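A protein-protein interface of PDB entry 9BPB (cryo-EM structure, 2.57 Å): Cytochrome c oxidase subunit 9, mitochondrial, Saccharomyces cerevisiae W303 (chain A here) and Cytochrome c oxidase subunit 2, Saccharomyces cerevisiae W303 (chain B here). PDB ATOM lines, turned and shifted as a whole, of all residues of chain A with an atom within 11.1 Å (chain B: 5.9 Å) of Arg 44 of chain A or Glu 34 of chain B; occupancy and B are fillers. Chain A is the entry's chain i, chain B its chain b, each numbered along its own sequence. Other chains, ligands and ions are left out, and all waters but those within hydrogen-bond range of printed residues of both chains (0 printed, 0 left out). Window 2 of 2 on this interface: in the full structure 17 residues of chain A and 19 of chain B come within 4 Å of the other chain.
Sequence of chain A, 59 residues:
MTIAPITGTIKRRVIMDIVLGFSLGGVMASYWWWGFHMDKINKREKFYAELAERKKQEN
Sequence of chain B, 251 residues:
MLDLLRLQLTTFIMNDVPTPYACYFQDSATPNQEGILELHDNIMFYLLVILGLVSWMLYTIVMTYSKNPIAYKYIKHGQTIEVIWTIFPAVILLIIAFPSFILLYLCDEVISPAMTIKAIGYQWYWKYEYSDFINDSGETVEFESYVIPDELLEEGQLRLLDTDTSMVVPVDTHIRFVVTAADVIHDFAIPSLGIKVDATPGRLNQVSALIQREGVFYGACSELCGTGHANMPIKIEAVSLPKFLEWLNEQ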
ATOM      1  N   TRP A  33      12.810 -35.714  -4.001  1.00  0.00           N
ATOM      2  CA  TRP A  33      11.927 -34.556  -4.084  1.00  0.00           C
ATOM      3  C   TRP A  33      12.164 -33.597  -2.923  1.00  0.00           C
ATOM      4  O   TRP A  33      12.455 -32.415  -3.135  1.00  0.00           O
ATOM      5  CB  TRP A  33      10.467 -35.009  -4.119  1.00  0.00           C
ATOM      6  CG  TRP A  33       9.500 -33.892  -4.382  1.00  0.00           C
ATOM      7  CD1 TRP A  33       8.704 -33.268  -3.467  1.00  0.00           C
ATOM      8  CD2 TRP A  33       9.225 -33.266  -5.643  1.00  0.00           C
ATOM      9  NE1 TRP A  33       7.954 -32.293  -4.077  1.00  0.00           N
ATOM     10  CE2 TRP A  33       8.255 -32.272  -5.413  1.00  0.00           C
ATOM     11  CE3 TRP A  33       9.707 -33.450  -6.942  1.00  0.00           C
ATOM     12  CZ2 TRP A  33       7.757 -31.467  -6.433  1.00  0.00           C
ATOM     13  CZ3 TRP A  33       9.210 -32.647  -7.955  1.00  0.00           C
ATOM     14  CH2 TRP A  33       8.246 -31.669  -7.693  1.00  0.00           C
ATOM     15  N   PHE A  36      16.753 -33.426  -2.041  1.00  0.00           N
ATOM     16  CA  PHE A  36      17.599 -32.777  -3.037  1.00  0.00           C
ATOM     17  C   PHE A  36      16.860 -31.671  -3.783  1.00  0.00           C
ATOM     18  O   PHE A  36      17.283 -30.510  -3.762  1.00  0.00           O
ATOM     19  CB  PHE A  36      18.135 -33.809  -4.035  1.00  0.00           C
ATOM     20  CG  PHE A  36      19.049 -33.223  -5.077  1.00  0.00           C
ATOM     21  CD1 PHE A  36      20.350 -32.877  -4.758  1.00  0.00           C
ATOM     22  CD2 PHE A  36      18.604 -33.004  -6.371  1.00  0.00           C
ATOM     23  CE1 PHE A  36      21.192 -32.331  -5.712  1.00  0.00           C
ATOM     24  CE2 PHE A  36      19.443 -32.458  -7.326  1.00  0.00           C
ATOM     25  CZ  PHE A  36      20.737 -32.122  -6.995  1.00  0.00           C
ATOM     26  N   HIS A  37      15.757 -32.019  -4.452  1.00  0.00           N
ATOM     27  CA  HIS A  37      15.087 -31.065  -5.331  1.00  0.00           C
ATOM     28  C   HIS A  37      14.531 -29.879  -4.554  1.00  0.00           C
ATOM     29  O   HIS A  37      14.609 -28.737  -5.022  1.00  0.00           O
ATOM     30  CB  HIS A  37      13.974 -31.760  -6.114  1.00  0.00           C
ATOM     31  CG  HIS A  37      13.056 -30.813  -6.824  1.00  0.00           C
ATOM     32  ND1 HIS A  37      13.515 -29.826  -7.668  1.00  0.00           N
ATOM     33  CD2 HIS A  37      11.707 -30.702  -6.813  1.00  0.00           C
ATOM     34  CE1 HIS A  37      12.487 -29.148  -8.149  1.00  0.00           C
ATOM     35  NE2 HIS A  37      11.379 -29.659  -7.646  1.00  0.00           N
ATOM     36  N   MET A  38      13.959 -30.123  -3.371  1.00  0.00           N
ATOM     37  CA  MET A  38      13.444 -29.013  -2.576  1.00  0.00           C
ATOM     38  C   MET A  38      14.565 -28.119  -2.067  1.00  0.00           C
ATOM     39  O   MET A  38      14.374 -26.905  -1.936  1.00  0.00           O
ATOM     40  CB  MET A  38      12.602 -29.531  -1.411  1.00  0.00           C
ATOM     41  CG  MET A  38      11.191 -29.932  -1.804  1.00  0.00           C
ATOM     42  SD  MET A  38      10.240 -28.565  -2.493  1.00  0.00           S
ATOM     43  CE  MET A  38       9.892 -27.619  -1.014  1.00  0.00           C
ATOM     44  N   ASP A  39      15.735 -28.694  -1.780  1.00  0.00           N
ATOM     45  CA  ASP A  39      16.883 -27.876  -1.404  1.00  0.00           C
ATOM     46  C   ASP A  39      17.285 -26.950  -2.543  1.00  0.00           C
ATOM     47  O   ASP A  39      17.647 -25.791  -2.313  1.00  0.00           O
ATOM     48  CB  ASP A  39      18.054 -28.771  -1.001  1.00  0.00           C
ATOM     49  CG  ASP A  39      19.096 -28.037  -0.179  1.00  0.00           C
ATOM     50  OD1 ASP A  39      19.037 -26.792  -0.103  1.00  0.00           O
ATOM     51  OD2 ASP A  39      19.980 -28.709   0.393  1.00  0.00           O
ATOM     52  N   LYS A  40      17.227 -27.447  -3.781  1.00  0.00           N
ATOM     53  CA  LYS A  40      17.602 -26.629  -4.928  1.00  0.00           C
ATOM     54  C   LYS A  40      16.672 -25.434  -5.089  1.00  0.00           C
ATOM     55  O   LYS A  40      17.119 -24.335  -5.432  1.00  0.00           O
ATOM     56  CB  LYS A  40      17.611 -27.481  -6.196  1.00  0.00           C
ATOM     57  CG  LYS A  40      18.921 -28.209  -6.436  1.00  0.00           C
ATOM     58  CD  LYS A  40      20.010 -27.236  -6.854  1.00  0.00           C
ATOM     59  CE  LYS A  40      21.396 -27.759  -6.508  1.00  0.00           C
ATOM     60  NZ  LYS A  40      21.677 -29.073  -7.147  1.00  0.00           N
ATOM     61  N   ILE A  41      15.373 -25.629  -4.851  1.00  0.00           N
ATOM     62  CA  ILE A  41      14.417 -24.543  -5.046  1.00  0.00           C
ATOM     63  C   ILE A  41      14.668 -23.413  -4.053  1.00  0.00           C
ATOM     64  O   ILE A  41      14.626 -22.231  -4.415  1.00  0.00           O
ATOM     65  CB  ILE A  41      12.975 -25.071  -4.944  1.00  0.00           C
ATOM     66  CG1 ILE A  41      12.689 -26.058  -6.073  1.00  0.00           C
ATOM     67  CG2 ILE A  41      11.980 -23.926  -4.992  1.00  0.00           C
ATOM     68  CD1 ILE A  41      11.380 -26.785  -5.907  1.00  0.00           C
ATOM     69  N   ASN A  42      14.928 -23.757  -2.789  1.00  0.00           N
ATOM     70  CA  ASN A  42      15.083 -22.732  -1.760  1.00  0.00           C
ATOM     71  C   ASN A  42      16.298 -21.851  -2.031  1.00  0.00           C
ATOM     72  O   ASN A  42      16.207 -20.619  -1.984  1.00  0.00           O
ATOM     73  CB  ASN A  42      15.185 -23.384  -0.383  1.00  0.00           C
ATOM     74  CG  ASN A  42      13.928 -24.139  -0.006  1.00  0.00           C
ATOM     75  OD1 ASN A  42      13.978 -25.317   0.347  1.00  0.00           O
ATOM     76  ND2 ASN A  42      12.786 -23.466  -0.087  1.00  0.00           N
ATOM     77  N   LYS A  43      17.449 -22.464  -2.316  1.00  0.00           N
ATOM     78  CA  LYS A  43      18.627 -21.678  -2.663  1.00  0.00           C
ATOM     79  C   LYS A  43      18.421 -20.903  -3.956  1.00  0.00           C
ATOM     80  O   LYS A  43      19.030 -19.845  -4.151  1.00  0.00           O
ATOM     81  CB  LYS A  43      19.856 -22.582  -2.771  1.00  0.00           C
ATOM     82  CG  LYS A  43      19.666 -23.791  -3.668  1.00  0.00           C
ATOM     83  CD  LYS A  43      20.936 -24.617  -3.759  1.00  0.00           C
ATOM     84  CE  LYS A  43      21.398 -25.065  -2.385  1.00  0.00           C
ATOM     85  NZ  LYS A  43      22.577 -25.970  -2.464  1.00  0.00           N
ATOM     86  N   ARG A  44      17.575 -21.415  -4.855  1.00  0.00           N
ATOM     87  CA  ARG A  44      17.226 -20.664  -6.055  1.00  0.00           C
ATOM     88  C   ARG A  44      16.409 -19.426  -5.710  1.00  0.00           C
ATOM     89  O   ARG A  44      16.666 -18.339  -6.239  1.00  0.00           O
ATOM     90  CB  ARG A  44      16.458 -21.559  -7.028  1.00  0.00           C
ATOM     91  CG  ARG A  44      17.339 -22.437  -7.897  1.00  0.00           C
ATOM     92  CD  ARG A  44      16.758 -22.603  -9.291  1.00  0.00           C
ATOM     93  NE  ARG A  44      15.419 -23.177  -9.266  1.00  0.00           N
ATOM     94  CZ  ARG A  44      14.315 -22.521  -9.597  1.00  0.00           C
ATOM     95  NH1 ARG A  44      14.350 -21.253  -9.974  1.00  0.00           N
ATOM     96  NH2 ARG A  44      13.146 -23.152  -9.548  1.00  0.00           N
ATOM     97  N   GLU A  45      15.427 -19.570  -4.816  1.00  0.00           N
ATOM     98  CA  GLU A  45      14.542 -18.456  -4.496  1.00  0.00           C
ATOM     99  C   GLU A  45      15.261 -17.364  -3.715  1.00  0.00           C
ATOM    100  O   GLU A  45      14.918 -16.186  -3.852  1.00  0.00           O
ATOM    101  CB  GLU A  45      13.333 -18.955  -3.709  1.00  0.00           C
ATOM    102  CG  GLU A  45      12.379 -19.810  -4.522  1.00  0.00           C
ATOM    103  CD  GLU A  45      11.058 -20.041  -3.813  1.00  0.00           C
ATOM    104  OE1 GLU A  45      10.890 -19.536  -2.684  1.00  0.00           O
ATOM    105  OE2 GLU A  45      10.188 -20.730  -4.386  1.00  0.00           O
ATOM    106  N   LYS A  46      16.248 -17.733  -2.896  1.00  0.00           N
ATOM    107  CA  LYS A  46      16.940 -16.746  -2.072  1.00  0.00           C
ATOM    108  C   LYS A  46      17.637 -15.695  -2.930  1.00  0.00           C
ATOM    109  O   LYS A  46      17.538 -14.493  -2.662  1.00  0.00           O
ATOM    110  CB  LYS A  46      17.945 -17.441  -1.154  1.00  0.00           C
ATOM    111  CG  LYS A  46      18.700 -16.494  -0.240  1.00  0.00           C
ATOM    112  CD  LYS A  46      19.698 -17.234   0.631  1.00  0.00           C
ATOM    113  CE  LYS A  46      20.506 -16.266   1.479  1.00  0.00           C
ATOM    114  NZ  LYS A  46      21.500 -16.964   2.336  1.00  0.00           N
ATOM    115  N   PHE A  47      18.347 -16.133  -3.972  1.00  0.00           N
ATOM    116  CA  PHE A  47      19.016 -15.185  -4.854  1.00  0.00           C
ATOM    117  C   PHE A  47      18.005 -14.316  -5.589  1.00  0.00           C
ATOM    118  O   PHE A  47      18.246 -13.124  -5.811  1.00  0.00           O
ATOM    119  CB  PHE A  47      19.911 -15.927  -5.848  1.00  0.00           C
ATOM    120  CG  PHE A  47      20.515 -15.042  -6.900  1.00  0.00           C
ATOM    121  CD1 PHE A  47      21.602 -14.240  -6.607  1.00  0.00           C
ATOM    122  CD2 PHE A  47      19.992 -15.007  -8.182  1.00  0.00           C
ATOM    123  CE1 PHE A  47      22.160 -13.420  -7.571  1.00  0.00           C
ATOM    124  CE2 PHE A  47      20.543 -14.190  -9.148  1.00  0.00           C
ATOM    125  CZ  PHE A  47      21.630 -13.396  -8.842  1.00  0.00           C
ATOM    126  N   TYR A  48      16.872 -14.900  -5.989  1.00  0.00           N
ATOM    127  CA  TYR A  48      15.811 -14.105  -6.598  1.00  0.00           C
ATOM    128  C   TYR A  48      15.120 -13.216  -5.572  1.00  0.00           C
ATOM    129  O   TYR A  48      14.678 -12.112  -5.910  1.00  0.00           O
ATOM    130  CB  TYR A  48      14.796 -15.016  -7.285  1.00  0.00           C
ATOM    131  CG  TYR A  48      15.294 -15.622  -8.578  1.00  0.00           C
ATOM    132  CD1 TYR A  48      15.583 -14.823  -9.676  1.00  0.00           C
ATOM    133  CD2 TYR A  48      15.474 -16.993  -8.699  1.00  0.00           C
ATOM    134  CE1 TYR A  48      16.039 -15.374 -10.858  1.00  0.00           C
ATOM    135  CE2 TYR A  48      15.931 -17.551  -9.875  1.00  0.00           C
ATOM    136  CZ  TYR A  48      16.212 -16.738 -10.952  1.00  0.00           C
ATOM    137  OH  TYR A  48      16.666 -17.295 -12.126  1.00  0.00           O
ATOM    138  N   ALA A  49      15.012 -13.680  -4.323  1.00  0.00           N
ATOM    139  CA  ALA A  49      14.424 -12.850  -3.276  1.00  0.00           C
ATOM    140  C   ALA A  49      15.252 -11.593  -3.039  1.00  0.00           C
ATOM    141  O   ALA A  49      14.701 -10.494  -2.909  1.00  0.00           O
ATOM    142  CB  ALA A  49      14.286 -13.651  -1.982  1.00  0.00           C
ATOM    143  N   GLU A  50      16.579 -11.735  -2.978  1.00  0.00           N
ATOM    144  CA  GLU A  50      17.440 -10.565  -2.851  1.00  0.00           C
ATOM    145  C   GLU A  50      17.361  -9.679  -4.086  1.00  0.00           C
ATOM    146  O   GLU A  50      17.522  -8.458  -3.983  1.00  0.00           O
ATOM    147  CB  GLU A  50      18.884 -11.003  -2.598  1.00  0.00           C
ATOM    148  CG  GLU A  50      19.830  -9.884  -2.173  1.00  0.00           C
ATOM    149  CD  GLU A  50      20.387  -9.097  -3.348  1.00  0.00           C
ATOM    150  OE1 GLU A  50      20.489  -9.669  -4.451  1.00  0.00           O
ATOM    151  OE2 GLU A  50      20.719  -7.907  -3.167  1.00  0.00           O
ATOM    152  N   LEU A  51      17.051 -10.297  -5.213  1.00  0.00           N
ATOM    153  CA  LEU A  51      16.901  -9.501  -6.445  1.00  0.00           C
ATOM    154  C   LEU A  51      15.720  -8.546  -6.244  1.00  0.00           C
ATOM    155  O   LEU A  51      15.967  -7.323  -6.264  1.00  0.00           O
ATOM    156  CB  LEU A  51      16.686 -10.474  -7.606  1.00  0.00           C
ATOM    157  CG  LEU A  51      17.964 -11.019  -8.239  1.00  0.00           C
ATOM    158  CD1 LEU A  51      17.649 -11.839  -9.481  1.00  0.00           C
ATOM    159  N   SER B  28      19.708 -22.055 -14.129  1.00  0.00           N
ATOM    160  CA  SER B  28      18.720 -21.506 -15.042  1.00  0.00           C
ATOM    161  C   SER B  28      18.853 -19.992 -15.141  1.00  0.00           C
ATOM    162  O   SER B  28      19.353 -19.326 -14.233  1.00  0.00           O
ATOM    163  CB  SER B  28      17.310 -21.867 -14.580  1.00  0.00           C
ATOM    164  OG  SER B  28      16.868 -20.978 -13.570  1.00  0.00           O
ATOM    165  N   THR B  30      16.129 -18.579 -17.436  1.00  0.00           N
ATOM    166  CA  THR B  30      14.891 -18.343 -18.157  1.00  0.00           C
ATOM    167  C   THR B  30      13.773 -19.145 -17.509  1.00  0.00           C
ATOM    168  O   THR B  30      14.024 -20.223 -16.955  1.00  0.00           O
ATOM    169  CB  THR B  30      15.014 -18.743 -19.637  1.00  0.00           C
ATOM    170  OG1 THR B  30      15.457 -20.104 -19.729  1.00  0.00           O
ATOM    171  CG2 THR B  30      16.012 -17.854 -20.365  1.00  0.00           C
ATOM    172  N   PRO B  31      12.535 -18.644 -17.552  1.00  0.00           N
ATOM    173  CA  PRO B  31      11.412 -19.420 -17.000  1.00  0.00           C
ATOM    174  C   PRO B  31      11.181 -20.750 -17.694  1.00  0.00           C
ATOM    175  O   PRO B  31      10.655 -21.677 -17.066  1.00  0.00           O
ATOM    176  CB  PRO B  31      10.211 -18.478 -17.180  1.00  0.00           C
ATOM    177  CG  PRO B  31      10.666 -17.442 -18.159  1.00  0.00           C
ATOM    178  CD  PRO B  31      12.122 -17.279 -17.909  1.00  0.00           C
ATOM    179  N   ASN B  32      11.541 -20.879 -18.972  1.00  0.00           N
ATOM    180  CA  ASN B  32      11.320 -22.148 -19.659  1.00  0.00           C
ATOM    181  C   ASN B  32      12.343 -23.193 -19.229  1.00  0.00           C
ATOM    182  O   ASN B  32      12.061 -24.395 -19.264  1.00  0.00           O
ATOM    183  CB  ASN B  32      11.344 -21.943 -21.175  1.00  0.00           C
ATOM    184  CG  ASN B  32      12.589 -21.224 -21.650  1.00  0.00           C
ATOM    185  OD1 ASN B  32      13.582 -21.134 -20.933  1.00  0.00           O
ATOM    186  ND2 ASN B  32      12.535 -20.693 -22.865  1.00  0.00           N
ATOM    187  N   GLN B  33      13.535 -22.752 -18.820  1.00  0.00           N
ATOM    188  CA  GLN B  33      14.528 -23.690 -18.305  1.00  0.00           C
ATOM    189  C   GLN B  33      14.140 -24.214 -16.931  1.00  0.00           C
ATOM    190  O   GLN B  33      14.479 -25.351 -16.583  1.00  0.00           O
ATOM    191  CB  GLN B  33      15.904 -23.023 -18.257  1.00  0.00           C
ATOM    192  CG  GLN B  33      17.055 -23.950 -17.869  1.00  0.00           C
ATOM    193  CD  GLN B  33      16.953 -25.332 -18.491  1.00  0.00           C
ATOM    194  OE1 GLN B  33      16.988 -26.341 -17.788  1.00  0.00           O
ATOM    195  NE2 GLN B  33      16.844 -25.384 -19.811  1.00  0.00           N
ATOM    196  N   GLU B  34      13.438 -23.404 -16.133  1.00  0.00           N
ATOM    197  CA  GLU B  34      12.914 -23.897 -14.865  1.00  0.00           C
ATOM    198  C   GLU B  34      11.882 -24.995 -15.091  1.00  0.00           C
ATOM    199  O   GLU B  34      11.901 -26.021 -14.401  1.00  0.00           O
ATOM    200  CB  GLU B  34      12.307 -22.748 -14.064  1.00  0.00           C
ATOM    201  CG  GLU B  34      13.312 -21.720 -13.593  1.00  0.00           C
ATOM    202  CD  GLU B  34      12.648 -20.507 -12.979  1.00  0.00           C
ATOM    203  OE1 GLU B  34      11.403 -20.429 -13.027  1.00  0.00           O
ATOM    204  OE2 GLU B  34      13.367 -19.630 -12.456  1.00  0.00           O
ATOM    205  N   GLY B  35      10.979 -24.799 -16.053  1.00  0.00           N
ATOM    206  CA  GLY B  35      10.035 -25.849 -16.390  1.00  0.00           C
ATOM    207  C   GLY B  35      10.723 -27.094 -16.912  1.00  0.00           C
ATOM    208  O   GLY B  35      10.306 -28.216 -16.617  1.00  0.00           O
ATOM    209  N   ILE B  36      11.782 -26.914 -17.701  1.00  0.00           N
ATOM    210  CA  ILE B  36      12.617 -28.044 -18.095  1.00  0.00           C
ATOM    211  C   ILE B  36      13.226 -28.700 -16.864  1.00  0.00           C
ATOM    212  O   ILE B  36      13.238 -29.929 -16.737  1.00  0.00           O
ATOM    213  CB  ILE B  36      13.698 -27.582 -19.090  1.00  0.00           C
ATOM    214  CG1 ILE B  36      13.089 -27.333 -20.471  1.00  0.00           C
ATOM    215  CG2 ILE B  36      14.823 -28.598 -19.179  1.00  0.00           C
ATOM    216  CD1 ILE B  36      13.814 -26.286 -21.275  1.00  0.00           C
ATOM    217  N   LEU B  37      13.737 -27.885 -15.936  1.00  0.00           N
ATOM    218  CA  LEU B  37      14.270 -28.413 -14.685  1.00  0.00           C
ATOM    219  C   LEU B  37      13.168 -29.023 -13.827  1.00  0.00           C
ATOM    220  O   LEU B  37      13.365 -30.077 -13.209  1.00  0.00           O
ATOM    221  CB  LEU B  37      15.003 -27.305 -13.926  1.00  0.00           C
ATOM    222  CG  LEU B  37      15.730 -27.628 -12.617  1.00  0.00           C
ATOM    223  CD1 LEU B  37      16.984 -26.780 -12.499  1.00  0.00           C
ATOM    224  CD2 LEU B  37      14.832 -27.388 -11.412  1.00  0.00           C
ATOM    225  N   GLU B  38      12.003 -28.374 -13.772  1.00  0.00           N
ATOM    226  CA  GLU B  38      10.915 -28.862 -12.927  1.00  0.00           C
ATOM    227  C   GLU B  38      10.313 -30.150 -13.477  1.00  0.00           C
ATOM    228  O   GLU B  38       9.989 -31.066 -12.711  1.00  0.00           O
ATOM    229  CB  GLU B  38       9.838 -27.785 -12.794  1.00  0.00           C
ATOM    230  CG  GLU B  38       8.681 -28.155 -11.884  1.00  0.00           C
ATOM    231  CD  GLU B  38       9.069 -28.150 -10.423  1.00  0.00           C
ATOM    232  OE1 GLU B  38      10.029 -27.440 -10.063  1.00  0.00           O
ATOM    233  OE2 GLU B  38       8.409 -28.855  -9.631  1.00  0.00           O
ATOM    234  N   LEU B  39      10.146 -30.235 -14.798  1.00  0.00           N
ATOM    235  CA  LEU B  39       9.561 -31.430 -15.394  1.00  0.00           C
ATOM    236  C   LEU B  39      10.472 -32.638 -15.227  1.00  0.00           C
ATOM    237  O   LEU B  39       9.994 -33.754 -14.999  1.00  0.00           O
ATOM    238  CB  LEU B  39       9.260 -31.190 -16.872  1.00  0.00           C
ATOM    239  CG  LEU B  39       8.464 -32.291 -17.572  1.00  0.00           C
ATOM    240  CD1 LEU B  39       7.004 -32.235 -17.165  1.00  0.00           C
ATOM    241  CD2 LEU B  39       8.611 -32.182 -19.079  1.00  0.00           C
ATOM    242  N   GLN B 212      16.251 -13.286 -17.051  1.00  0.00           N
ATOM    243  CA  GLN B 212      15.867 -12.645 -15.801  1.00  0.00           C
ATOM    244  C   GLN B 212      17.041 -12.348 -14.873  1.00  0.00           C
ATOM    245  O   GLN B 212      16.814 -11.959 -13.722  1.00  0.00           O
ATOM    246  CB  GLN B 212      14.839 -13.512 -15.068  1.00  0.00           C
ATOM    247  CG  GLN B 212      15.152 -15.001 -15.120  1.00  0.00           C
ATOM    248  CD  GLN B 212      13.979 -15.867 -14.708  1.00  0.00           C
ATOM    249  OE1 GLN B 212      12.864 -15.381 -14.527  1.00  0.00           O
ATOM    250  NE2 GLN B 212      14.225 -17.161 -14.558  1.00  0.00           N
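Among the printed residues, pairs that only touch across the chains: Trp 33 of chain A with Glu 38 of chain B, His 37 of chain A with Glu 38 of chain B and Tyr 48 of chain A with Ser 28 of chain B.
Of chain B, only Glu 34 (3.1 Å) comes within 4 Å of Arg 44 of chain A. Of chain A, only Arg 44 comes within 4 Å of Glu 34 of chain B. Gln 33 of chain B touches none of the printed residues of chain A. Gly 35 of chain B touches none of the printed residues of chain A. No residue of chain A comes within 4 Å of Leu 37 of chain B. Of the printed residues of chain B, Tyr 48 of chain A touches Ser 28 and Gln 212. Of the printed residues of chain A, Gln 212 of chain B touches Tyr 48 (3.4 Å). Of the printed residues of chain B, Trp 33 of chain A touches Glu 38. The nearest residue of chain B that does not touch Arg 44 of chain A is Ser 28 of chain B (4.4 Å). The nearest residue of chain A that does not touch Glu 34 of chain B is Tyr 48 of chain A (4.1 Å). The nearest printed residue of chain B that does not touch Tyr 48 of chain A is Glu 34 of chain B (4.1 Å).
The side-chain amide nitrogen (NE2) of Gln 212 of chain B lies within hydrogen-bond range of the side-chain hydroxyl (OH) of Tyr 48 of chain A. The side-chain carboxylate of Glu 34 of chain B lies within salt-bridge range of the guanidinium group of Arg 44 of chain A, at 3.1 Å.
The side-chain carboxylate (OE2) of Glu 34 of chain B sits at hydrogen-bond distance from the side-chain amide nitrogen (NE2) of Gln 212 of chain B (3.4 Å). O of Trp 33 of chain A lies within hydrogen-bond range of N of Met 38 of chain A, at 2.8 Å.
Of the 17 printed residues of chain A, 4 touch a printed residue of chain B. Hydrophobic or aromatic side chains of chain A within 4 Å of the printed part of chain B: Trp 33, His 37 and Tyr 48. Among the printed residues, Asp or Glu carboxylates within 4 Å of a Lys or Arg side-chain nitrogen of the other chain: Arg 44 of chain A with Glu 34 of chain B (3.1 Å).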
